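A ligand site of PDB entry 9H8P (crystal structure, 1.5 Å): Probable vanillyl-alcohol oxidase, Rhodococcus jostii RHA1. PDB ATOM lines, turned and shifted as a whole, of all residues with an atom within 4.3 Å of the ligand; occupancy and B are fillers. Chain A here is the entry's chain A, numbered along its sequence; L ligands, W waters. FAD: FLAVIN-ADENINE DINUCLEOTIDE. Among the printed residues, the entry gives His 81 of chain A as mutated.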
ATOM      1  N   TYR A  44       3.911  -6.354  18.631  1.00  0.00           N
ATOM      2  CA  TYR A  44       4.364  -7.664  19.056  1.00  0.00           C
ATOM      3  C   TYR A  44       3.408  -8.160  20.140  1.00  0.00           C
ATOM      4  O   TYR A  44       3.722  -8.227  21.320  1.00  0.00           O
ATOM      5  CB  TYR A  44       5.805  -7.574  19.594  1.00  0.00           C
ATOM      6  CG  TYR A  44       6.865  -6.981  18.669  1.00  0.00           C
ATOM      7  CD1 TYR A  44       6.719  -6.883  17.293  1.00  0.00           C
ATOM      8  CD2 TYR A  44       8.021  -6.430  19.243  1.00  0.00           C
ATOM      9  CE1 TYR A  44       7.721  -6.331  16.507  1.00  0.00           C
ATOM     10  CE2 TYR A  44       9.007  -5.885  18.453  1.00  0.00           C
ATOM     11  CZ  TYR A  44       8.856  -5.810  17.084  1.00  0.00           C
ATOM     12  OH  TYR A  44       9.783  -5.269  16.232  1.00  0.00           O
ATOM     13  N   HIS A  81      -2.914   7.336  28.331  1.00  0.00           N
ATOM     14  CA  HIS A  81      -1.639   6.623  28.329  1.00  0.00           C
ATOM     15  C   HIS A  81      -0.648   7.524  27.616  1.00  0.00           C
ATOM     16  O   HIS A  81      -0.659   7.615  26.396  1.00  0.00           O
ATOM     17  CB  HIS A  81      -1.747   5.304  27.601  1.00  0.00           C
ATOM     18  CG  HIS A  81      -0.472   4.549  27.423  1.00  0.00           C
ATOM     19  ND1 HIS A  81       0.366   4.272  28.465  1.00  0.00           N
ATOM     20  CD2 HIS A  81       0.138   4.035  26.334  1.00  0.00           C
ATOM     21  CE1 HIS A  81       1.431   3.601  27.982  1.00  0.00           C
ATOM     22  NE2 HIS A  81       1.288   3.438  26.711  1.00  0.00           N
ATOM     23  N   PRO A  82       0.224   8.240  28.346  1.00  0.00           N
ATOM     24  CA  PRO A  82       1.173   9.108  27.696  1.00  0.00           C
ATOM     25  C   PRO A  82       2.365   8.340  27.157  1.00  0.00           C
ATOM     26  O   PRO A  82       2.907   7.467  27.848  1.00  0.00           O
ATOM     27  CB  PRO A  82       1.662  10.033  28.833  1.00  0.00           C
ATOM     28  CG  PRO A  82       1.540   9.164  30.071  1.00  0.00           C
ATOM     29  CD  PRO A  82       0.266   8.328  29.819  1.00  0.00           C
ATOM     30  N   VAL A  83       2.756   8.692  25.932  1.00  0.00           N
ATOM     31  CA  VAL A  83       3.971   8.154  25.332  1.00  0.00           C
ATOM     32  C   VAL A  83       4.732   9.319  24.736  1.00  0.00           C
ATOM     33  O   VAL A  83       4.221  10.426  24.619  1.00  0.00           O
ATOM     34  CB  VAL A  83       3.677   7.059  24.286  1.00  0.00           C
ATOM     35  CG1 VAL A  83       2.776   5.969  24.855  1.00  0.00           C
ATOM     36  CG2 VAL A  83       3.054   7.645  23.022  1.00  0.00           C
ATOM     37  N   SER A  84       5.978   9.027  24.335  1.00  0.00           N
ATOM     38  CA  SER A  84       6.812   9.975  23.635  1.00  0.00           C
ATOM     39  C   SER A  84       6.769   9.679  22.147  1.00  0.00           C
ATOM     40  O   SER A  84       5.963  10.272  21.456  1.00  0.00           O
ATOM     41  CB  SER A  84       8.228   9.969  24.243  1.00  0.00           C
ATOM     42  OG  SER A  84       8.226  10.477  25.571  1.00  0.00           O
ATOM     43  N   THR A  85       7.523   8.676  21.705  1.00  0.00           N
ATOM     44  CA  THR A  85       7.466   8.159  20.346  1.00  0.00           C
ATOM     45  C   THR A  85       6.669   6.854  20.267  1.00  0.00           C
ATOM     46  O   THR A  85       6.317   6.461  19.166  1.00  0.00           O
ATOM     47  CB  THR A  85       8.881   8.049  19.759  1.00  0.00           C
ATOM     48  OG1 THR A  85       9.752   7.516  20.738  1.00  0.00           O
ATOM     49  CG2 THR A  85       9.413   9.413  19.370  1.00  0.00           C
ATOM     50  N   GLY A  86       6.391   6.183  21.396  1.00  0.00           N
ATOM     51  CA  GLY A  86       5.553   4.989  21.368  1.00  0.00           C
ATOM     52  C   GLY A  86       6.218   3.772  20.702  1.00  0.00           C
ATOM     53  O   GLY A  86       5.524   2.967  20.091  1.00  0.00           O
ATOM     54  N   LYS A  87       7.538   3.684  20.837  1.00  0.00           N
ATOM     55  CA  LYS A  87       8.314   2.617  20.220  1.00  0.00           C
ATOM     56  C   LYS A  87       8.785   1.595  21.257  1.00  0.00           C
ATOM     57  O   LYS A  87       9.803   0.936  21.076  1.00  0.00           O
ATOM     58  CB  LYS A  87       9.525   3.105  19.422  1.00  0.00           C
ATOM     59  CG  LYS A  87       9.224   4.048  18.303  1.00  0.00           C
ATOM     60  CD  LYS A  87       8.465   3.371  17.213  1.00  0.00           C
ATOM     61  CE  LYS A  87       8.952   3.624  15.784  1.00  0.00           C
ATOM     62  NZ  LYS A  87       8.434   2.560  14.923  1.00  0.00           N
ATOM     63  N   ASN A  88       8.014   1.393  22.347  1.00  0.00           N
ATOM     64  CA  ASN A  88       8.389   0.533  23.447  1.00  0.00           C
ATOM     65  C   ASN A  88       8.133  -0.941  23.101  1.00  0.00           C
ATOM     66  O   ASN A  88       7.515  -1.713  23.857  1.00  0.00           O
ATOM     67  CB  ASN A  88       7.621   0.946  24.707  1.00  0.00           C
ATOM     68  CG  ASN A  88       8.357   0.620  26.009  1.00  0.00           C
ATOM     69  OD1 ASN A  88       9.612   0.523  25.972  1.00  0.00           O
ATOM     70  ND2 ASN A  88       7.641   0.507  27.118  1.00  0.00           N
ATOM     71  N   ASN A  89       8.688  -1.327  21.948  1.00  0.00           N
ATOM     72  CA  ASN A  89       8.406  -2.632  21.369  1.00  0.00           C
ATOM     73  C   ASN A  89       9.181  -3.684  22.163  1.00  0.00           C
ATOM     74  O   ASN A  89      10.343  -3.490  22.501  1.00  0.00           O
ATOM     75  CB  ASN A  89       8.830  -2.641  19.931  1.00  0.00           C
ATOM     76  CG  ASN A  89       8.055  -1.659  19.102  1.00  0.00           C
ATOM     77  OD1 ASN A  89       6.972  -1.213  19.471  1.00  0.00           O
ATOM     78  ND2 ASN A  89       8.547  -1.425  17.896  1.00  0.00           N
ATOM     79  N   GLY A  93       4.768  -1.686  22.921  1.00  0.00           N
ATOM     80  CA  GLY A  93       4.728  -0.668  21.888  1.00  0.00           C
ATOM     81  C   GLY A  93       4.101   0.592  22.446  1.00  0.00           C
ATOM     82  O   GLY A  93       4.452   0.986  23.547  1.00  0.00           O
ATOM     83  N   THR A 106       2.880  12.530  22.877  1.00  0.00           N
ATOM     84  CA  THR A 106       3.505  13.824  23.084  1.00  0.00           C
ATOM     85  C   THR A 106       4.543  14.115  22.015  1.00  0.00           C
ATOM     86  O   THR A 106       4.711  15.289  21.618  1.00  0.00           O
ATOM     87  CB  THR A 106       4.100  13.960  24.491  1.00  0.00           C
ATOM     88  OG1 THR A 106       5.155  12.993  24.641  1.00  0.00           O
ATOM     89  CG2 THR A 106       3.076  13.878  25.571  1.00  0.00           C
ATOM     90  N   PRO A 127       9.722  15.384  24.216  1.00  0.00           N
ATOM     91  CA  PRO A 127       9.615  13.940  24.059  1.00  0.00           C
ATOM     92  C   PRO A 127       9.811  13.371  22.656  1.00  0.00           C
ATOM     93  O   PRO A 127      10.163  12.195  22.488  1.00  0.00           O
ATOM     94  CB  PRO A 127       8.250  13.583  24.632  1.00  0.00           C
ATOM     95  CG  PRO A 127       7.986  14.753  25.554  1.00  0.00           C
ATOM     96  CD  PRO A 127       8.514  15.947  24.846  1.00  0.00           C
ATOM     97  N   PRO A 150      20.035   3.241  23.030  1.00  0.00           N
ATOM     98  CA  PRO A 150      19.735   1.830  23.089  1.00  0.00           C
ATOM     99  C   PRO A 150      20.037   1.179  21.726  1.00  0.00           C
ATOM    100  O   PRO A 150      20.576   1.821  20.820  1.00  0.00           O
ATOM    101  CB  PRO A 150      18.281   1.820  23.456  1.00  0.00           C
ATOM    102  CG  PRO A 150      17.750   3.051  22.747  1.00  0.00           C
ATOM    103  CD  PRO A 150      18.852   4.083  22.856  1.00  0.00           C
ATOM    104  N   ASP A 151      19.725  -0.107  21.609  1.00  0.00           N
ATOM    105  CA  ASP A 151      20.066  -0.838  20.392  1.00  0.00           C
ATOM    106  C   ASP A 151      19.420  -0.253  19.122  1.00  0.00           C
ATOM    107  O   ASP A 151      20.002  -0.363  18.041  1.00  0.00           O
ATOM    108  CB  ASP A 151      19.618  -2.280  20.499  1.00  0.00           C
ATOM    109  CG  ASP A 151      20.559  -3.177  21.297  1.00  0.00           C
ATOM    110  OD1 ASP A 151      21.575  -2.662  21.804  1.00  0.00           O
ATOM    111  OD2 ASP A 151      20.114  -4.299  21.614  1.00  0.00           O
ATOM    112  N   LEU A 152      18.219   0.306  19.232  1.00  0.00           N
ATOM    113  CA  LEU A 152      17.493   0.877  18.108  1.00  0.00           C
ATOM    114  C   LEU A 152      17.400   2.390  18.257  1.00  0.00           C
ATOM    115  O   LEU A 152      17.026   2.893  19.325  1.00  0.00           O
ATOM    116  CB  LEU A 152      16.099   0.253  18.028  1.00  0.00           C
ATOM    117  CG  LEU A 152      16.077  -1.262  17.883  1.00  0.00           C
ATOM    118  CD1 LEU A 152      14.641  -1.774  18.022  1.00  0.00           C
ATOM    119  CD2 LEU A 152      16.707  -1.723  16.563  1.00  0.00           C
ATOM    120  N   GLY A 155      13.646   5.354  18.838  1.00  0.00           N
ATOM    121  CA  GLY A 155      12.905   5.787  20.010  1.00  0.00           C
ATOM    122  C   GLY A 155      13.373   7.158  20.493  1.00  0.00           C
ATOM    123  O   GLY A 155      14.121   7.875  19.842  1.00  0.00           O
ATOM    124  N   SER A 156      12.837   7.504  21.660  1.00  0.00           N
ATOM    125  CA  SER A 156      12.883   8.825  22.230  1.00  0.00           C
ATOM    126  C   SER A 156      13.920   8.869  23.333  1.00  0.00           C
ATOM    127  O   SER A 156      13.905   8.043  24.276  1.00  0.00           O
ATOM    128  CB  SER A 156      11.510   9.186  22.828  1.00  0.00           C
ATOM    129  OG  SER A 156      11.608  10.346  23.647  1.00  0.00           O
ATOM    130  N   GLY A 159      11.430   9.285  26.266  1.00  0.00           N
ATOM    131  CA  GLY A 159      10.555   8.149  26.527  1.00  0.00           C
ATOM    132  C   GLY A 159      11.316   6.934  27.050  1.00  0.00           C
ATOM    133  O   GLY A 159      10.886   6.249  27.952  1.00  0.00           O
ATOM    134  N   ASN A 160      12.478   6.659  26.434  1.00  0.00           N
ATOM    135  CA  ASN A 160      13.325   5.570  26.875  1.00  0.00           C
ATOM    136  C   ASN A 160      13.699   5.754  28.335  1.00  0.00           C
ATOM    137  O   ASN A 160      13.570   4.826  29.140  1.00  0.00           O
ATOM    138  CB  ASN A 160      14.550   5.475  25.968  1.00  0.00           C
ATOM    139  CG  ASN A 160      15.458   4.376  26.389  1.00  0.00           C
ATOM    140  OD1 ASN A 160      16.227   4.544  27.338  1.00  0.00           O
ATOM    141  ND2 ASN A 160      15.340   3.229  25.748  1.00  0.00           N
ATOM    142  N   LEU A 162      12.168   7.431  30.600  1.00  0.00           N
ATOM    143  CA  LEU A 162      11.023   7.347  31.462  1.00  0.00           C
ATOM    144  C   LEU A 162      10.585   5.887  31.697  1.00  0.00           C
ATOM    145  O   LEU A 162       9.790   5.672  32.633  1.00  0.00           O
ATOM    146  CB  LEU A 162       9.852   8.173  30.931  1.00  0.00           C
ATOM    147  CG  LEU A 162      10.146   9.672  30.882  1.00  0.00           C
ATOM    148  CD1 LEU A 162       8.942  10.395  30.272  1.00  0.00           C
ATOM    149  CD2 LEU A 162      10.511  10.262  32.252  1.00  0.00           C
ATOM    150  N   ASP A 163      11.068   4.909  30.934  1.00  0.00           N
ATOM    151  CA  ASP A 163      10.864   3.519  31.292  1.00  0.00           C
ATOM    152  C   ASP A 163      12.126   2.871  31.879  1.00  0.00           C
ATOM    153  O   ASP A 163      12.167   1.664  32.006  1.00  0.00           O
ATOM    154  CB  ASP A 163      10.324   2.735  30.106  1.00  0.00           C
ATOM    155  CG  ASP A 163       9.323   1.660  30.425  1.00  0.00           C
ATOM    156  OD1 ASP A 163       8.552   1.900  31.433  1.00  0.00           O
ATOM    157  OD2 ASP A 163       9.252   0.627  29.720  1.00  0.00           O
ATOM    158  N   GLY A 165      15.049   2.835  30.482  1.00  0.00           N
ATOM    159  CA  GLY A 165      15.827   2.224  29.445  1.00  0.00           C
ATOM    160  C   GLY A 165      17.308   2.528  29.554  1.00  0.00           C
ATOM    161  O   GLY A 165      17.760   3.367  30.337  1.00  0.00           O
ATOM    162  N   VAL A 166      18.067   1.798  28.721  1.00  0.00           N
ATOM    163  CA  VAL A 166      19.500   1.733  28.902  1.00  0.00           C
ATOM    164  C   VAL A 166      20.215   1.668  27.571  1.00  0.00           C
ATOM    165  O   VAL A 166      19.700   1.187  26.566  1.00  0.00           O
ATOM    166  CB  VAL A 166      19.885   0.498  29.753  1.00  0.00           C
ATOM    167  CG1 VAL A 166      19.332   0.594  31.152  1.00  0.00           C
ATOM    168  CG2 VAL A 166      19.509  -0.775  29.065  1.00  0.00           C
ATOM    169  N   TYR A 168      24.783   1.685  26.250  1.00  0.00           N
ATOM    170  CA  TYR A 168      25.976   0.836  26.376  1.00  0.00           C
ATOM    171  C   TYR A 168      27.269   1.630  26.473  1.00  0.00           C
ATOM    172  O   TYR A 168      28.337   1.003  26.607  1.00  0.00           O
ATOM    173  CB  TYR A 168      26.052  -0.194  25.242  1.00  0.00           C
ATOM    174  CG  TYR A 168      24.777  -1.019  25.217  1.00  0.00           C
ATOM    175  CD1 TYR A 168      24.607  -2.128  26.045  1.00  0.00           C
ATOM    176  CD2 TYR A 168      23.703  -0.593  24.463  1.00  0.00           C
ATOM    177  CE1 TYR A 168      23.416  -2.840  26.040  1.00  0.00           C
ATOM    178  CE2 TYR A 168      22.485  -1.270  24.500  1.00  0.00           C
ATOM    179  CZ  TYR A 168      22.334  -2.342  25.348  1.00  0.00           C
ATOM    180  OH  TYR A 168      21.131  -3.012  25.389  1.00  0.00           O
ATOM    181  N   GLY A 225       2.140  11.273  35.921  1.00  0.00           N
ATOM    182  CA  GLY A 225       2.053  12.486  35.148  1.00  0.00           C
ATOM    183  C   GLY A 225       2.378  12.282  33.681  1.00  0.00           C
ATOM    184  O   GLY A 225       2.690  11.158  33.271  1.00  0.00           O
ATOM    185  N   ILE A 226       2.306  13.380  32.931  1.00  0.00           N
ATOM    186  CA  ILE A 226       2.698  13.419  31.540  1.00  0.00           C
ATOM    187  C   ILE A 226       3.893  14.364  31.435  1.00  0.00           C
ATOM    188  O   ILE A 226       3.776  15.585  31.669  1.00  0.00           O
ATOM    189  CB  ILE A 226       1.542  13.860  30.637  1.00  0.00           C
ATOM    190  CG1 ILE A 226       0.326  12.965  30.837  1.00  0.00           C
ATOM    191  CG2 ILE A 226       2.019  13.921  29.182  1.00  0.00           C
ATOM    192  CD1 ILE A 226      -0.824  13.248  29.890  1.00  0.00           C
ATOM    193  N   VAL A 227       5.070  13.814  31.142  1.00  0.00           N
ATOM    194  CA  VAL A 227       6.306  14.594  31.069  1.00  0.00           C
ATOM    195  C   VAL A 227       6.361  15.348  29.756  1.00  0.00           C
ATOM    196  O   VAL A 227       6.044  14.789  28.663  1.00  0.00           O
ATOM    197  CB  VAL A 227       7.521  13.677  31.218  1.00  0.00           C
ATOM    198  CG1 VAL A 227       8.836  14.391  30.905  1.00  0.00           C
ATOM    199  CG2 VAL A 227       7.529  13.015  32.611  1.00  0.00           C
ATOM    200  N   LEU A 381      16.799  -8.930  13.727  1.00  0.00           N
ATOM    201  CA  LEU A 381      16.422 -10.000  14.665  1.00  0.00           C
ATOM    202  C   LEU A 381      15.007 -10.499  14.397  1.00  0.00           C
ATOM    203  O   LEU A 381      14.728 -11.698  14.529  1.00  0.00           O
ATOM    204  CB  LEU A 381      16.507  -9.558  16.130  1.00  0.00           C
ATOM    205  CG  LEU A 381      17.900  -9.324  16.694  1.00  0.00           C
ATOM    206  CD1 LEU A 381      17.740  -8.635  18.044  1.00  0.00           C
ATOM    207  CD2 LEU A 381      18.698 -10.575  16.898  1.00  0.00           C
ATOM    208  N   HIS A 390       8.981  -9.717  19.299  1.00  0.00           N
ATOM    209  CA  HIS A 390       9.673 -10.194  20.498  1.00  0.00           C
ATOM    210  C   HIS A 390       8.979  -9.658  21.746  1.00  0.00           C
ATOM    211  O   HIS A 390       8.256  -8.664  21.704  1.00  0.00           O
ATOM    212  CB  HIS A 390      11.151  -9.850  20.458  1.00  0.00           C
ATOM    213  CG  HIS A 390      11.496  -8.416  20.631  1.00  0.00           C
ATOM    214  ND1 HIS A 390      11.386  -7.782  21.857  1.00  0.00           N
ATOM    215  CD2 HIS A 390      11.956  -7.479  19.780  1.00  0.00           C
ATOM    216  CE1 HIS A 390      11.781  -6.539  21.728  1.00  0.00           C
ATOM    217  NE2 HIS A 390      12.150  -6.280  20.493  1.00  0.00           N
ATOM    218  N   LEU A 438      15.309 -12.359  25.080  1.00  0.00           N
ATOM    219  CA  LEU A 438      14.382 -11.934  24.044  1.00  0.00           C
ATOM    220  C   LEU A 438      13.758 -13.231  23.500  1.00  0.00           C
ATOM    221  O   LEU A 438      14.483 -14.170  23.209  1.00  0.00           O
ATOM    222  CB  LEU A 438      15.241 -11.280  22.935  1.00  0.00           C
ATOM    223  CG  LEU A 438      14.647 -10.123  22.145  1.00  0.00           C
ATOM    224  CD1 LEU A 438      14.283  -8.995  23.098  1.00  0.00           C
ATOM    225  CD2 LEU A 438      15.664  -9.644  21.152  1.00  0.00           C
ATOM    226  N   ARG A 472      12.004  -4.292  34.372  1.00  0.00           N
ATOM    227  CA  ARG A 472      11.122  -3.650  33.386  1.00  0.00           C
ATOM    228  C   ARG A 472      10.331  -4.805  32.767  1.00  0.00           C
ATOM    229  O   ARG A 472      10.819  -5.923  32.650  1.00  0.00           O
ATOM    230  CB  ARG A 472      11.988  -2.995  32.300  1.00  0.00           C
ATOM    231  CG  ARG A 472      11.290  -2.081  31.312  1.00  0.00           C
ATOM    232  CD  ARG A 472      12.357  -1.433  30.446  1.00  0.00           C
ATOM    233  NE  ARG A 472      11.841  -0.588  29.365  1.00  0.00           N
ATOM    234  CZ  ARG A 472      12.572  -0.134  28.395  1.00  0.00           C
ATOM    235  NH1 ARG A 472      13.860  -0.420  28.359  1.00  0.00           N
ATOM    236  NH2 ARG A 472      12.007   0.613  27.458  1.00  0.00           N
ATOM    237  N   LYS A 513      -0.161   0.753  34.910  1.00  0.00           N
ATOM    238  CA  LYS A 513       1.278   0.819  34.632  1.00  0.00           C
ATOM    239  C   LYS A 513       2.029   0.334  35.863  1.00  0.00           C
ATOM    240  O   LYS A 513       1.726   0.739  37.006  1.00  0.00           O
ATOM    241  CB  LYS A 513       1.698   2.258  34.327  1.00  0.00           C
ATOM    242  CG  LYS A 513       3.183   2.498  34.160  1.00  0.00           C
ATOM    243  CD  LYS A 513       3.794   1.732  32.999  1.00  0.00           C
ATOM    244  CE  LYS A 513       5.281   2.004  32.898  1.00  0.00           C
ATOM    245  NZ  LYS A 513       5.911   1.157  31.863  1.00  0.00           N
HETATM  246  PA  FAD L   1       7.941   5.360  24.550  1.00  0.00           P
HETATM  247  O1A FAD L   1       7.292   4.149  23.995  1.00  0.00           O
HETATM  248  O2A FAD L   1       7.484   6.666  24.051  1.00  0.00           O
HETATM  249  O5B FAD L   1       7.766   5.400  26.139  1.00  0.00           O
HETATM  250  C5B FAD L   1       7.989   4.276  26.991  1.00  0.00           C
HETATM  251  C4B FAD L   1       7.080   4.319  28.217  1.00  0.00           C
HETATM  252  O4B FAD L   1       7.545   5.425  29.017  1.00  0.00           O
HETATM  253  C3B FAD L   1       5.614   4.651  27.958  1.00  0.00           C
HETATM  254  O3B FAD L   1       4.918   3.466  27.654  1.00  0.00           O
HETATM  255  C2B FAD L   1       5.228   5.290  29.246  1.00  0.00           C
HETATM  256  O2B FAD L   1       4.945   4.283  30.215  1.00  0.00           O
HETATM  257  C1B FAD L   1       6.429   6.166  29.535  1.00  0.00           C
HETATM  258  N9A FAD L   1       6.355   7.496  28.938  1.00  0.00           N
HETATM  259  C8A FAD L   1       6.944   7.874  27.776  1.00  0.00           C
HETATM  260  N7A FAD L   1       6.801   9.129  27.478  1.00  0.00           N
HETATM  261  C5A FAD L   1       6.072   9.628  28.556  1.00  0.00           C
HETATM  262  C6A FAD L   1       5.723  10.953  28.837  1.00  0.00           C
HETATM  263  N6A FAD L   1       5.968  11.961  28.033  1.00  0.00           N
HETATM  264  N1A FAD L   1       5.106  11.148  30.016  1.00  0.00           N
HETATM  265  C2A FAD L   1       4.906  10.100  30.790  1.00  0.00           C
HETATM  266  N3A FAD L   1       5.164   8.777  30.644  1.00  0.00           N
HETATM  267  C4A FAD L   1       5.827   8.637  29.477  1.00  0.00           C
HETATM  268  N1  FAD L   1      15.376  -0.792  25.125  1.00  0.00           N
HETATM  269  C2  FAD L   1      16.419  -0.318  25.854  1.00  0.00           C
HETATM  270  O2  FAD L   1      16.250   0.469  26.801  1.00  0.00           O
HETATM  271  N3  FAD L   1      17.703  -0.684  25.452  1.00  0.00           N
HETATM  272  C4  FAD L   1      17.977  -1.564  24.450  1.00  0.00           C
HETATM  273  O4  FAD L   1      19.139  -1.717  24.102  1.00  0.00           O
HETATM  274  C4X FAD L   1      16.889  -2.054  23.746  1.00  0.00           C
HETATM  275  N5  FAD L   1      17.093  -2.896  22.730  1.00  0.00           N
HETATM  276  C5X FAD L   1      15.975  -3.413  22.106  1.00  0.00           C
HETATM  277  C6  FAD L   1      16.172  -4.337  21.054  1.00  0.00           C
HETATM  278  C7  FAD L   1      15.121  -4.889  20.377  1.00  0.00           C
HETATM  279  C7M FAD L   1      15.368  -5.878  19.261  1.00  0.00           C
HETATM  280  C8  FAD L   1      13.805  -4.443  20.657  1.00  0.00           C
HETATM  281  C8M FAD L   1      12.657  -4.975  19.856  1.00  0.00           C
HETATM  282  C9  FAD L   1      13.607  -3.493  21.649  1.00  0.00           C
HETATM  283  C9A FAD L   1      14.692  -2.960  22.373  1.00  0.00           C
HETATM  284  N10 FAD L   1      14.511  -2.025  23.400  1.00  0.00           N
HETATM  285  C10 FAD L   1      15.604  -1.591  24.122  1.00  0.00           C
HETATM  286  C1' FAD L   1      13.145  -1.570  23.775  1.00  0.00           C
HETATM  287  C2' FAD L   1      12.711  -0.309  23.020  1.00  0.00           C
HETATM  288  O2' FAD L   1      13.174  -0.361  21.645  1.00  0.00           O
HETATM  289  C3' FAD L   1      13.391   0.999  23.528  1.00  0.00           C
HETATM  290  O3' FAD L   1      13.432   1.068  24.964  1.00  0.00           O
HETATM  291  C4' FAD L   1      12.693   2.289  23.087  1.00  0.00           C
HETATM  292  O4' FAD L   1      13.574   3.415  23.107  1.00  0.00           O
HETATM  293  C5' FAD L   1      11.443   2.560  23.936  1.00  0.00           C
HETATM  294  O5' FAD L   1      10.437   3.317  23.160  1.00  0.00           O
HETATM  295  P   FAD L   1      10.387   4.870  23.136  1.00  0.00           P
HETATM  296  O1P FAD L   1       9.550   5.278  21.935  1.00  0.00           O
HETATM  297  O2P FAD L   1      11.762   5.433  23.309  1.00  0.00           O
HETATM  298  O3P FAD L   1       9.538   5.220  24.479  1.00  0.00           O
HETATM  299  O   HOH W   1       3.629   6.981  32.168  1.00  0.00           O
HETATM  300  O   HOH W   2       4.379   1.367  29.486  1.00  0.00           O
HETATM  301  O   HOH W   3       4.902   3.400  24.930  1.00  0.00           O
HETATM  302  O   HOH W   4      16.078   0.070  21.419  1.00  0.00           O
HETATM  303  O   HOH W   5       7.328   4.362  32.001  1.00  0.00           O
HETATM  304  O   HOH W   6      11.654  -0.415  19.296  1.00  0.00           O
HETATM  305  O   HOH W   7      14.790   3.407  20.474  1.00  0.00           O
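A carbon (C8M) of the ligand is covalently linked to a ring nitrogen (NE2) of His 390 (1.5 Å).
An oxygen (O2A) of the ligand sits at hydrogen-bond distance from the backbone NH of Thr 85 (3.1 Å).
An oxygen (O1P) of the ligand is in hydrogen-bond range of the side-chain hydroxyl of Thr 85, 2.5 Å away.
The side-chain hydroxyl (OH) of Tyr 168 lies within hydrogen-bond range of an oxygen (O4) of the ligand, 2.7 Å away.
An oxygen (O2A) of the ligand is in hydrogen-bond range of the backbone NH (N) of Ser 84, 2.8 Å away.
The side-chain hydroxyl (OG) of Ser 84 is in hydrogen-bond range of a nitrogen (N7A) of the ligand (2.7 Å).
The backbone NH (N) of Lys 87 lies within hydrogen-bond range of an oxygen (O1P) of the ligand (2.8 Å).
N of Ser 156 is in hydrogen-bond range of O2P of the ligand, 2.9 Å away.
A nitrogen (N1A) of the ligand is in hydrogen-bond range of the backbone NH (N) of Val 227 (2.9 Å).
A nitrogen (N6A) of the ligand is in hydrogen-bond range of the backbone carbonyl oxygen of Val 227, at 2.9 Å.
An oxygen (O3') of the ligand is in hydrogen-bond range of the guanidinium group (NH2) of Arg 472 (2.9 Å).
An oxygen (O2A) of the ligand lies within hydrogen-bond range of the backbone NH (N) of Gly 86.
N of Val 166 lies within hydrogen-bond range of O2 of the ligand (3.0 Å).
A nitrogen (N3) of the ligand is in hydrogen-bond range of the backbone carbonyl oxygen of Val 166, 3.0 Å away.
N of Asn 160 sits at hydrogen-bond distance from O2P of the ligand.
The side-chain amide nitrogen (ND2) of Asn 160 sits at hydrogen-bond distance from an oxygen (O3') of the ligand (3.0 Å).
O4 of the ligand sits at hydrogen-bond distance from N of Asp 151 (3.0 Å).
An oxygen (O5') of the ligand sits at hydrogen-bond distance from the backbone NH (N) of Asn 88.
The side-chain hydroxyl (OG) of Ser 156 is in hydrogen-bond range of the backbone NH (N) of Gly 159 (2.8 Å).
The backbone carbonyl oxygen (O) of Pro 127 is in hydrogen-bond range of the side-chain hydroxyl (OG) of Ser 156, 2.6 Å away.
NH2 of Arg 472 is in hydrogen-bond range of OD1 of Asn 88.
The guanidinium group of Arg 472 lies within salt-bridge range of the side-chain carboxylate of Asp 163, at 2.9 Å.
The backbone NH (N) of Gly 165 lies within hydrogen-bond range of the backbone carbonyl oxygen (O) of Asn 160, at 2.8 Å.
ND2 of Asn 88 lies within hydrogen-bond range of OD2 of Asp 163.
The backbone carbonyl oxygen (O) of Asn 88 is in hydrogen-bond range of the backbone NH (N) of Gly 93, at 2.9 Å.
The backbone carbonyl oxygen (O) of Val 83 lies within hydrogen-bond range of the side-chain hydroxyl (OG1) of Thr 106.
Water W3 bridges O1A of the ligand and O of Gly 93.
Water W6 bridges an oxygen (O2') of the ligand (2.8 Å) and the backbone carbonyl oxygen (O) of Lys 87 (2.9 Å).
Water W2 lies within hydrogen-bond range of NZ of Lys 513 (2.8 Å) and O3B of the ligand (2.8 Å).
Water W7 lies within hydrogen-bond range of O of Leu 152 (2.6 Å), N of Gly 155 (2.8 Å) and O4' of the ligand (2.9 Å).
Water W4 bridges O2' of the ligand and N of Leu 152.
Water W5 lies within hydrogen-bond range of OD1 of Asp 163 (2.8 Å), O of Leu 162 (2.9 Å) and O2B of the ligand (3.0 Å).
His 81 touches the ligand.
Pro 82 touches the ligand.
Val 83 touches the ligand (C to N7A, 3.4 Å).
Asn 89 touches the ligand.
Thr 106 touches the ligand.
CB of Pro 150 touches N3 of the ligand, at 3.3 Å.
CD1 of Leu 152 touches C8 of the ligand, at 3.8 Å.
CA of Gly 155 touches O2P of the ligand, at 3.5 Å.
Gly 159 touches the ligand.
Leu 162 touches the ligand.
Gly 165 touches the ligand.
Gly 225 touches the ligand (O to C2A, 3.5 Å).
Ile 226 touches the ligand (CA to N1A, 3.6 Å).
CD1 of Leu 381 touches C7M of the ligand (3.8 Å).
CE of Lys 513 touches O2B of the ligand, at 3.5 Å.
Hydrophobic or aromatic side chains that line the ligand: His 81, Pro 82, Val 83, Pro 150, Leu 152, Leu 162, Tyr 168, Val 227, Leu 381 and His 390.
Of the 33 residues printed, 28 come within 4 Å of the ligand.
Along chain A the residues within 4 Å of the ligand span positions 81 to 513.
The nearest printed residue that does not touch the ligand is Tyr 44 (4.01 Å).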
